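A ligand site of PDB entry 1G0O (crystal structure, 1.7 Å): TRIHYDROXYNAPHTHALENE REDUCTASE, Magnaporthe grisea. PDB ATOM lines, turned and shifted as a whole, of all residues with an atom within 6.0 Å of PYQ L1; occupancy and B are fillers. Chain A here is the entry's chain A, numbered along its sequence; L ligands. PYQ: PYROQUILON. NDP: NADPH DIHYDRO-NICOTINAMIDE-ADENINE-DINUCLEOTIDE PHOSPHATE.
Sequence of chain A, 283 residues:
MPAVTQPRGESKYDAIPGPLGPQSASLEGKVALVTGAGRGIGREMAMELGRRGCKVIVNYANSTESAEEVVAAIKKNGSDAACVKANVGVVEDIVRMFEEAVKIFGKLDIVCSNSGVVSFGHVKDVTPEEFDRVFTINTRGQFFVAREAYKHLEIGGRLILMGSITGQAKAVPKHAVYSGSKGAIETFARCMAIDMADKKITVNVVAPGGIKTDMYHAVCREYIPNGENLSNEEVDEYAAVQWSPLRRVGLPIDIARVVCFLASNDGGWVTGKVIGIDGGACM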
ATOM      1  N   VAL A 118      20.025  24.633  -2.265  1.00  0.00           N
ATOM      2  CA  VAL A 118      18.745  24.007  -2.521  1.00  0.00           C
ATOM      3  C   VAL A 118      18.641  22.678  -1.757  1.00  0.00           C
ATOM      4  O   VAL A 118      19.642  22.136  -1.272  1.00  0.00           O
ATOM      5  CB  VAL A 118      18.524  23.816  -4.064  1.00  0.00           C
ATOM      6  CG1 VAL A 118      19.437  22.709  -4.607  1.00  0.00           C
ATOM      7  CG2 VAL A 118      17.059  23.558  -4.400  1.00  0.00           C
ATOM      8  N   GLY A 163      14.850  35.596  -3.466  1.00  0.00           N
ATOM      9  CA  GLY A 163      13.779  34.667  -3.144  1.00  0.00           C
ATOM     10  C   GLY A 163      13.779  33.586  -4.211  1.00  0.00           C
ATOM     11  O   GLY A 163      14.838  33.223  -4.762  1.00  0.00           O
ATOM     12  N   SER A 164      12.583  33.125  -4.574  1.00  0.00           N
ATOM     13  CA  SER A 164      12.406  32.101  -5.585  1.00  0.00           C
ATOM     14  C   SER A 164      10.923  31.943  -5.884  1.00  0.00           C
ATOM     15  O   SER A 164      10.085  32.267  -5.043  1.00  0.00           O
ATOM     16  CB  SER A 164      12.935  30.764  -5.078  1.00  0.00           C
ATOM     17  OG  SER A 164      12.641  29.728  -5.998  1.00  0.00           O
ATOM     18  N   ILE A 165      10.603  31.406  -7.065  1.00  0.00           N
ATOM     19  CA  ILE A 165       9.216  31.135  -7.443  1.00  0.00           C
ATOM     20  C   ILE A 165       8.616  30.154  -6.422  1.00  0.00           C
ATOM     21  O   ILE A 165       7.410  30.112  -6.202  1.00  0.00           O
ATOM     22  CB  ILE A 165       9.129  30.536  -8.891  1.00  0.00           C
ATOM     23  CG1 ILE A 165       7.670  30.421  -9.358  1.00  0.00           C
ATOM     24  CG2 ILE A 165       9.801  29.163  -8.960  1.00  0.00           C
ATOM     25  CD1 ILE A 165       7.532  30.152 -10.835  1.00  0.00           C
ATOM     26  N   THR A 166       9.497  29.383  -5.766  1.00  0.00           N
ATOM     27  CA  THR A 166       9.082  28.391  -4.765  1.00  0.00           C
ATOM     28  C   THR A 166       8.417  29.007  -3.524  1.00  0.00           C
ATOM     29  O   THR A 166       7.674  28.330  -2.809  1.00  0.00           O
ATOM     30  CB  THR A 166      10.259  27.472  -4.357  1.00  0.00           C
ATOM     31  OG1 THR A 166      11.282  28.263  -3.736  1.00  0.00           O
ATOM     32  CG2 THR A 166      10.863  26.752  -5.586  1.00  0.00           C
ATOM     33  N   HIS A 175       9.457  19.666  -1.232  1.00  0.00           N
ATOM     34  CA  HIS A 175      10.208  20.914  -1.307  1.00  0.00           C
ATOM     35  C   HIS A 175       9.911  21.902  -0.172  1.00  0.00           C
ATOM     36  O   HIS A 175      10.214  23.082  -0.264  1.00  0.00           O
ATOM     37  CB  HIS A 175       9.873  21.599  -2.629  1.00  0.00           C
ATOM     38  CG  HIS A 175      11.032  22.372  -3.255  1.00  0.00           C
ATOM     39  ND1 HIS A 175      12.337  21.971  -3.104  1.00  0.00           N
ATOM     40  CD2 HIS A 175      11.044  23.490  -3.997  1.00  0.00           C
ATOM     41  CE1 HIS A 175      13.119  22.819  -3.743  1.00  0.00           C
ATOM     42  NE2 HIS A 175      12.366  23.755  -4.290  1.00  0.00           N
ATOM     43  N   TYR A 178      13.240  24.148   1.427  1.00  0.00           N
ATOM     44  CA  TYR A 178      13.781  25.170   0.545  1.00  0.00           C
ATOM     45  C   TYR A 178      12.747  26.249   0.230  1.00  0.00           C
ATOM     46  O   TYR A 178      13.048  27.434   0.289  1.00  0.00           O
ATOM     47  CB  TYR A 178      14.275  24.540  -0.742  1.00  0.00           C
ATOM     48  CG  TYR A 178      14.780  25.548  -1.766  1.00  0.00           C
ATOM     49  CD1 TYR A 178      16.055  26.104  -1.665  1.00  0.00           C
ATOM     50  CD2 TYR A 178      13.972  25.918  -2.853  1.00  0.00           C
ATOM     51  CE1 TYR A 178      16.531  26.999  -2.619  1.00  0.00           C
ATOM     52  CE2 TYR A 178      14.436  26.811  -3.812  1.00  0.00           C
ATOM     53  CZ  TYR A 178      15.707  27.343  -3.687  1.00  0.00           C
ATOM     54  OH  TYR A 178      16.169  28.196  -4.665  1.00  0.00           O
ATOM     55  N   LYS A 182      12.714  30.415   1.363  1.00  0.00           N
ATOM     56  CA  LYS A 182      12.577  31.483   0.369  1.00  0.00           C
ATOM     57  C   LYS A 182      11.332  32.351   0.586  1.00  0.00           C
ATOM     58  O   LYS A 182      11.366  33.572   0.353  1.00  0.00           O
ATOM     59  CB  LYS A 182      12.564  30.885  -1.054  1.00  0.00           C
ATOM     60  CG  LYS A 182      13.909  30.247  -1.491  1.00  0.00           C
ATOM     61  CD  LYS A 182      15.047  31.265  -1.483  1.00  0.00           C
ATOM     62  CE  LYS A 182      16.281  30.747  -2.176  1.00  0.00           C
ATOM     63  NZ  LYS A 182      17.315  31.804  -2.277  1.00  0.00           N
ATOM     64  N   PRO A 208      13.251  34.460  -8.917  1.00  0.00           N
ATOM     65  CA  PRO A 208      13.424  33.812 -10.216  1.00  0.00           C
ATOM     66  C   PRO A 208      12.712  32.476 -10.368  1.00  0.00           C
ATOM     67  O   PRO A 208      12.391  31.793  -9.384  1.00  0.00           O
ATOM     68  CB  PRO A 208      14.946  33.556 -10.269  1.00  0.00           C
ATOM     69  CG  PRO A 208      15.531  34.495  -9.242  1.00  0.00           C
ATOM     70  CD  PRO A 208      14.502  34.446  -8.151  1.00  0.00           C
ATOM     71  N   GLY A 209      12.447  32.117 -11.623  1.00  0.00           N
ATOM     72  CA  GLY A 209      11.908  30.808 -11.946  1.00  0.00           C
ATOM     73  C   GLY A 209      13.198  30.020 -12.181  1.00  0.00           C
ATOM     74  O   GLY A 209      14.266  30.487 -11.787  1.00  0.00           O
ATOM     75  N   GLY A 210      13.127  28.841 -12.803  1.00  0.00           N
ATOM     76  CA  GLY A 210      14.335  28.084 -13.060  1.00  0.00           C
ATOM     77  C   GLY A 210      15.301  28.863 -13.952  1.00  0.00           C
ATOM     78  O   GLY A 210      14.896  29.413 -14.978  1.00  0.00           O
ATOM     79  N   ILE A 211      16.571  28.899 -13.555  1.00  0.00           N
ATOM     80  CA  ILE A 211      17.626  29.625 -14.290  1.00  0.00           C
ATOM     81  C   ILE A 211      18.816  28.667 -14.481  1.00  0.00           C
ATOM     82  O   ILE A 211      19.239  28.019 -13.517  1.00  0.00           O
ATOM     83  CB  ILE A 211      18.128  30.846 -13.470  1.00  0.00           C
ATOM     84  CG1 ILE A 211      16.979  31.793 -13.118  1.00  0.00           C
ATOM     85  CG2 ILE A 211      19.224  31.561 -14.208  1.00  0.00           C
ATOM     86  CD1 ILE A 211      16.326  32.481 -14.287  1.00  0.00           C
ATOM     87  N   MET A 215      23.158  24.986  -9.900  1.00  0.00           N
ATOM     88  CA  MET A 215      22.037  24.537  -9.084  1.00  0.00           C
ATOM     89  C   MET A 215      20.969  23.881  -9.962  1.00  0.00           C
ATOM     90  O   MET A 215      20.474  22.791  -9.645  1.00  0.00           O
ATOM     91  CB  MET A 215      21.428  25.720  -8.322  1.00  0.00           C
ATOM     92  CG  MET A 215      20.312  25.293  -7.365  1.00  0.00           C
ATOM     93  SD  MET A 215      19.613  26.642  -6.386  1.00  0.00           S
ATOM     94  CE  MET A 215      21.013  27.014  -5.224  1.00  0.00           C
ATOM     95  N   TYR A 216      20.620  24.541 -11.069  1.00  0.00           N
ATOM     96  CA  TYR A 216      19.636  24.041 -12.025  1.00  0.00           C
ATOM     97  C   TYR A 216      20.088  22.652 -12.527  1.00  0.00           C
ATOM     98  O   TYR A 216      19.306  21.694 -12.557  1.00  0.00           O
ATOM     99  CB  TYR A 216      19.533  25.046 -13.185  1.00  0.00           C
ATOM    100  CG  TYR A 216      18.733  24.613 -14.403  1.00  0.00           C
ATOM    101  CD1 TYR A 216      17.426  25.081 -14.604  1.00  0.00           C
ATOM    102  CD2 TYR A 216      19.311  23.838 -15.411  1.00  0.00           C
ATOM    103  CE1 TYR A 216      16.740  24.803 -15.796  1.00  0.00           C
ATOM    104  CE2 TYR A 216      18.630  23.563 -16.595  1.00  0.00           C
ATOM    105  CZ  TYR A 216      17.352  24.048 -16.781  1.00  0.00           C
ATOM    106  OH  TYR A 216      16.675  23.758 -17.950  1.00  0.00           O
ATOM    107  N   VAL A 219      19.511  19.968  -9.757  1.00  0.00           N
ATOM    108  CA  VAL A 219      18.164  19.572  -9.329  1.00  0.00           C
ATOM    109  C   VAL A 219      16.954  19.828 -10.224  1.00  0.00           C
ATOM    110  O   VAL A 219      15.826  19.530  -9.817  1.00  0.00           O
ATOM    111  CB  VAL A 219      17.842  20.169  -7.954  1.00  0.00           C
ATOM    112  CG1 VAL A 219      18.884  19.747  -6.917  1.00  0.00           C
ATOM    113  CG2 VAL A 219      17.775  21.699  -8.069  1.00  0.00           C
ATOM    114  N   CYS A 220      17.160  20.319 -11.441  1.00  0.00           N
ATOM    115  CA  CYS A 220      16.033  20.603 -12.326  1.00  0.00           C
ATOM    116  C   CYS A 220      15.074  19.434 -12.493  1.00  0.00           C
ATOM    117  O   CYS A 220      13.860  19.629 -12.519  1.00  0.00           O
ATOM    118  CB  CYS A 220      16.461  21.099 -13.691  1.00  0.00           C
ATOM    119  SG  CYS A 220      15.030  21.670 -14.662  1.00  0.00           S
ATOM    120  N   TYR A 223      11.999  18.855 -10.220  1.00  0.00           N
ATOM    121  CA  TYR A 223      10.815  19.688 -10.461  1.00  0.00           C
ATOM    122  C   TYR A 223       9.961  19.098 -11.580  1.00  0.00           C
ATOM    123  O   TYR A 223       8.880  19.632 -11.885  1.00  0.00           O
ATOM    124  CB  TYR A 223      11.227  21.107 -10.863  1.00  0.00           C
ATOM    125  CG  TYR A 223      11.893  21.927  -9.765  1.00  0.00           C
ATOM    126  CD1 TYR A 223      13.284  21.953  -9.629  1.00  0.00           C
ATOM    127  CD2 TYR A 223      11.123  22.700  -8.881  1.00  0.00           C
ATOM    128  CE1 TYR A 223      13.896  22.716  -8.648  1.00  0.00           C
ATOM    129  CE2 TYR A 223      11.717  23.464  -7.892  1.00  0.00           C
ATOM    130  CZ  TYR A 223      13.110  23.473  -7.773  1.00  0.00           C
ATOM    131  OH  TYR A 223      13.714  24.247  -6.816  1.00  0.00           O
ATOM    132  N   TRP A 243       7.479  25.752 -18.468  1.00  0.00           N
ATOM    133  CA  TRP A 243       7.542  26.893 -17.558  1.00  0.00           C
ATOM    134  C   TRP A 243       7.493  28.300 -18.158  1.00  0.00           C
ATOM    135  O   TRP A 243       7.675  29.273 -17.443  1.00  0.00           O
ATOM    136  CB  TRP A 243       8.729  26.732 -16.611  1.00  0.00           C
ATOM    137  CG  TRP A 243       8.664  25.467 -15.796  1.00  0.00           C
ATOM    138  CD1 TRP A 243       7.535  24.840 -15.325  1.00  0.00           C
ATOM    139  CD2 TRP A 243       9.770  24.648 -15.374  1.00  0.00           C
ATOM    140  NE1 TRP A 243       7.873  23.691 -14.645  1.00  0.00           N
ATOM    141  CE2 TRP A 243       9.238  23.549 -14.662  1.00  0.00           C
ATOM    142  CE3 TRP A 243      11.163  24.745 -15.524  1.00  0.00           C
ATOM    143  CZ2 TRP A 243      10.049  22.550 -14.116  1.00  0.00           C
ATOM    144  CZ3 TRP A 243      11.978  23.741 -14.966  1.00  0.00           C
ATOM    145  CH2 TRP A 243      11.418  22.665 -14.275  1.00  0.00           C
ATOM    146  N   MET A 283       4.188  27.245 -11.398  1.00  0.00           N
ATOM    147  CA  MET A 283       4.762  26.093 -10.695  1.00  0.00           C
ATOM    148  C   MET A 283       4.121  25.833  -9.306  1.00  0.00           C
ATOM    149  O   MET A 283       4.337  24.735  -8.756  1.00  0.00           O
ATOM    150  CB  MET A 283       6.283  26.269 -10.549  1.00  0.00           C
ATOM    151  CG  MET A 283       7.019  26.327 -11.887  1.00  0.00           C
ATOM    152  SD  MET A 283       8.822  26.359 -11.727  1.00  0.00           S
ATOM    153  CE  MET A 283       9.170  24.642 -11.183  1.00  0.00           C
ATOM    154  OXT MET A 283       3.425  26.735  -8.788  1.00  0.00           O
HETATM  155  C1  PYQ L   1      13.281  25.123 -11.530  1.00  0.00           C
HETATM  156  C2  PYQ L   1      13.457  25.894 -10.368  1.00  0.00           C
HETATM  157  C3  PYQ L   1      14.705  25.792  -9.717  1.00  0.00           C
HETATM  158  C5  PYQ L   1      15.734  24.985 -10.166  1.00  0.00           C
HETATM  159  C6  PYQ L   1      16.905  25.138  -9.211  1.00  0.00           C
HETATM  160  C7  PYQ L   1      16.332  26.160  -8.177  1.00  0.00           C
HETATM  161  N8  PYQ L   1      15.038  26.458  -8.594  1.00  0.00           N
HETATM  162  C9  PYQ L   1      14.169  27.286  -8.027  1.00  0.00           C
HETATM  163  O10 PYQ L   1      14.517  27.908  -6.963  1.00  0.00           O
HETATM  164  C11 PYQ L   1      12.885  27.469  -8.601  1.00  0.00           C
HETATM  165  C12 PYQ L   1      12.526  26.770  -9.780  1.00  0.00           C
HETATM  166  C13 PYQ L   1      15.561  24.217 -11.319  1.00  0.00           C
HETATM  167  C14 PYQ L   1      14.321  24.288 -11.995  1.00  0.00           C
HETATM  168  PA  NDP L   2      24.649  27.853  -7.388  1.00  0.00           P
HETATM  169  O1A NDP L   2      25.109  27.868  -8.806  1.00  0.00           O
HETATM  170  O2A NDP L   2      24.384  26.606  -6.643  1.00  0.00           O
HETATM  171  O5B NDP L   2      25.675  28.778  -6.530  1.00  0.00           O
HETATM  172  C5B NDP L   2      25.076  29.758  -5.655  1.00  0.00           C
HETATM  173  C4B NDP L   2      26.022  30.639  -4.848  1.00  0.00           C
HETATM  174  O4B NDP L   2      25.705  30.486  -3.439  1.00  0.00           O
HETATM  175  C3B NDP L   2      27.477  30.274  -5.061  1.00  0.00           C
HETATM  176  O3B NDP L   2      28.274  31.422  -5.373  1.00  0.00           O
HETATM  177  C2B NDP L   2      27.941  29.863  -3.686  1.00  0.00           C
HETATM  178  O2B NDP L   2      29.349  30.252  -3.530  1.00  0.00           O
HETATM  179  C1B NDP L   2      26.961  30.624  -2.808  1.00  0.00           C
HETATM  180  N9A NDP L   2      27.055  30.159  -1.420  1.00  0.00           N
HETATM  181  C8A NDP L   2      26.615  28.964  -0.992  1.00  0.00           C
HETATM  182  N7A NDP L   2      26.822  28.845   0.309  1.00  0.00           N
HETATM  183  C5A NDP L   2      27.398  29.975   0.665  1.00  0.00           C
HETATM  184  C6A NDP L   2      27.800  30.318   1.971  1.00  0.00           C
HETATM  185  N6A NDP L   2      27.654  29.498   3.026  1.00  0.00           N
HETATM  186  N1A NDP L   2      28.376  31.555   2.108  1.00  0.00           N
HETATM  187  C2A NDP L   2      28.524  32.397   1.054  1.00  0.00           C
HETATM  188  N3A NDP L   2      28.120  32.043  -0.199  1.00  0.00           N
HETATM  189  C4A NDP L   2      27.560  30.840  -0.416  1.00  0.00           C
HETATM  190  O3  NDP L   2      23.345  28.774  -7.306  1.00  0.00           O
HETATM  191  PN  NDP L   2      22.506  29.693  -8.275  1.00  0.00           P
HETATM  192  O1N NDP L   2      23.467  30.648  -8.852  1.00  0.00           O
HETATM  193  O2N NDP L   2      21.650  28.876  -9.148  1.00  0.00           O
HETATM  194  O5D NDP L   2      21.546  30.461  -7.245  1.00  0.00           O
HETATM  195  C5D NDP L   2      21.912  31.693  -6.602  1.00  0.00           C
HETATM  196  C4D NDP L   2      20.744  32.183  -5.739  1.00  0.00           C
HETATM  197  O4D NDP L   2      19.513  32.263  -6.529  1.00  0.00           O
HETATM  198  C3D NDP L   2      20.421  31.207  -4.623  1.00  0.00           C
HETATM  199  O3D NDP L   2      20.070  31.922  -3.435  1.00  0.00           O
HETATM  200  C2D NDP L   2      19.272  30.357  -5.163  1.00  0.00           C
HETATM  201  O2D NDP L   2      18.485  29.724  -4.165  1.00  0.00           O
HETATM  202  C1D NDP L   2      18.520  31.393  -5.950  1.00  0.00           C
HETATM  203  N1N NDP L   2      17.677  30.823  -7.047  1.00  0.00           N
HETATM  204  C2N NDP L   2      18.201  30.007  -8.072  1.00  0.00           C
HETATM  205  C3N NDP L   2      17.352  29.536  -9.078  1.00  0.00           C
HETATM  206  C7N NDP L   2      17.830  28.640 -10.248  1.00  0.00           C
HETATM  207  O7N NDP L   2      17.008  28.056 -10.939  1.00  0.00           O
HETATM  208  N7N NDP L   2      19.162  28.518 -10.458  1.00  0.00           N
HETATM  209  C4N NDP L   2      15.974  29.887  -9.046  1.00  0.00           C
HETATM  210  C5N NDP L   2      15.447  30.691  -8.026  1.00  0.00           C
HETATM  211  C6N NDP L   2      16.295  31.171  -7.024  1.00  0.00           C
HETATM  212  P2B NDP L   2      30.527  29.211  -3.272  1.00  0.00           P
HETATM  213  O1X NDP L   2      30.967  28.656  -4.553  1.00  0.00           O
HETATM  214  O2X NDP L   2      30.162  28.168  -2.296  1.00  0.00           O
HETATM  215  O3X NDP L   2      31.674  29.991  -2.772  1.00  0.00           O
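OG of Ser 164 lies within hydrogen-bond range of OG1 of Thr 166, at 3.0 Å.
A ring nitrogen (NE2) of His 175 lies within hydrogen-bond range of the side-chain hydroxyl (OH) of Tyr 223, at 2.9 Å.
The backbone NH (N) of Ile 165 is in hydrogen-bond range of the backbone carbonyl oxygen (O) of Pro 208, 3.0 Å away.
O2D of NDP L2 is in hydrogen-bond range of OH of Tyr 178, 2.8 Å away.
O3D of NDP L2 sits at hydrogen-bond distance from NZ of Lys 182 (3.0 Å).
An oxygen (O10) of PYQ L1 is in hydrogen-bond range of the side-chain hydroxyl (OG) of Ser 164, 2.8 Å away.
The backbone carbonyl oxygen (O) of Ile 211 sits at hydrogen-bond distance from a nitrogen (N7N) of NDP L2.
OH of Tyr 178 is in hydrogen-bond range of O10 of PYQ L1 (2.8 Å).
An oxygen (O7N) of NDP L2 lies within hydrogen-bond range of the backbone NH (N) of Ile 211 (2.8 Å).
OH of Tyr 223 lies close to N8 of PYQ L1 (3.1 Å).
Ile 165 touches PYQ L1.
Thr 166 touches PYQ L1 (CG2 to C11, 3.7 Å).
Gly 210 touches PYQ L1 (CA to C1, 3.5 Å).
Met 215 touches PYQ L1 (SD to C7, 3.8 Å).
Tyr 216 touches PYQ L1.
Val 219 touches PYQ L1 (CG2 to C6, 3.7 Å).
CA of Cys 220 touches C13 of PYQ L1, 3.8 Å away.
Trp 243 touches PYQ L1.
11 residues have an atom within 4 Å of PYQ L1: Ser 164, Ile 165, Thr 166, Tyr 178, Gly 210, Met 215, Tyr 216, Val 219, Cys 220, Tyr 223 and Trp 243.
The nearest printed residue that does not touch PYQ L1 is Gly 209 (4.1 Å).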
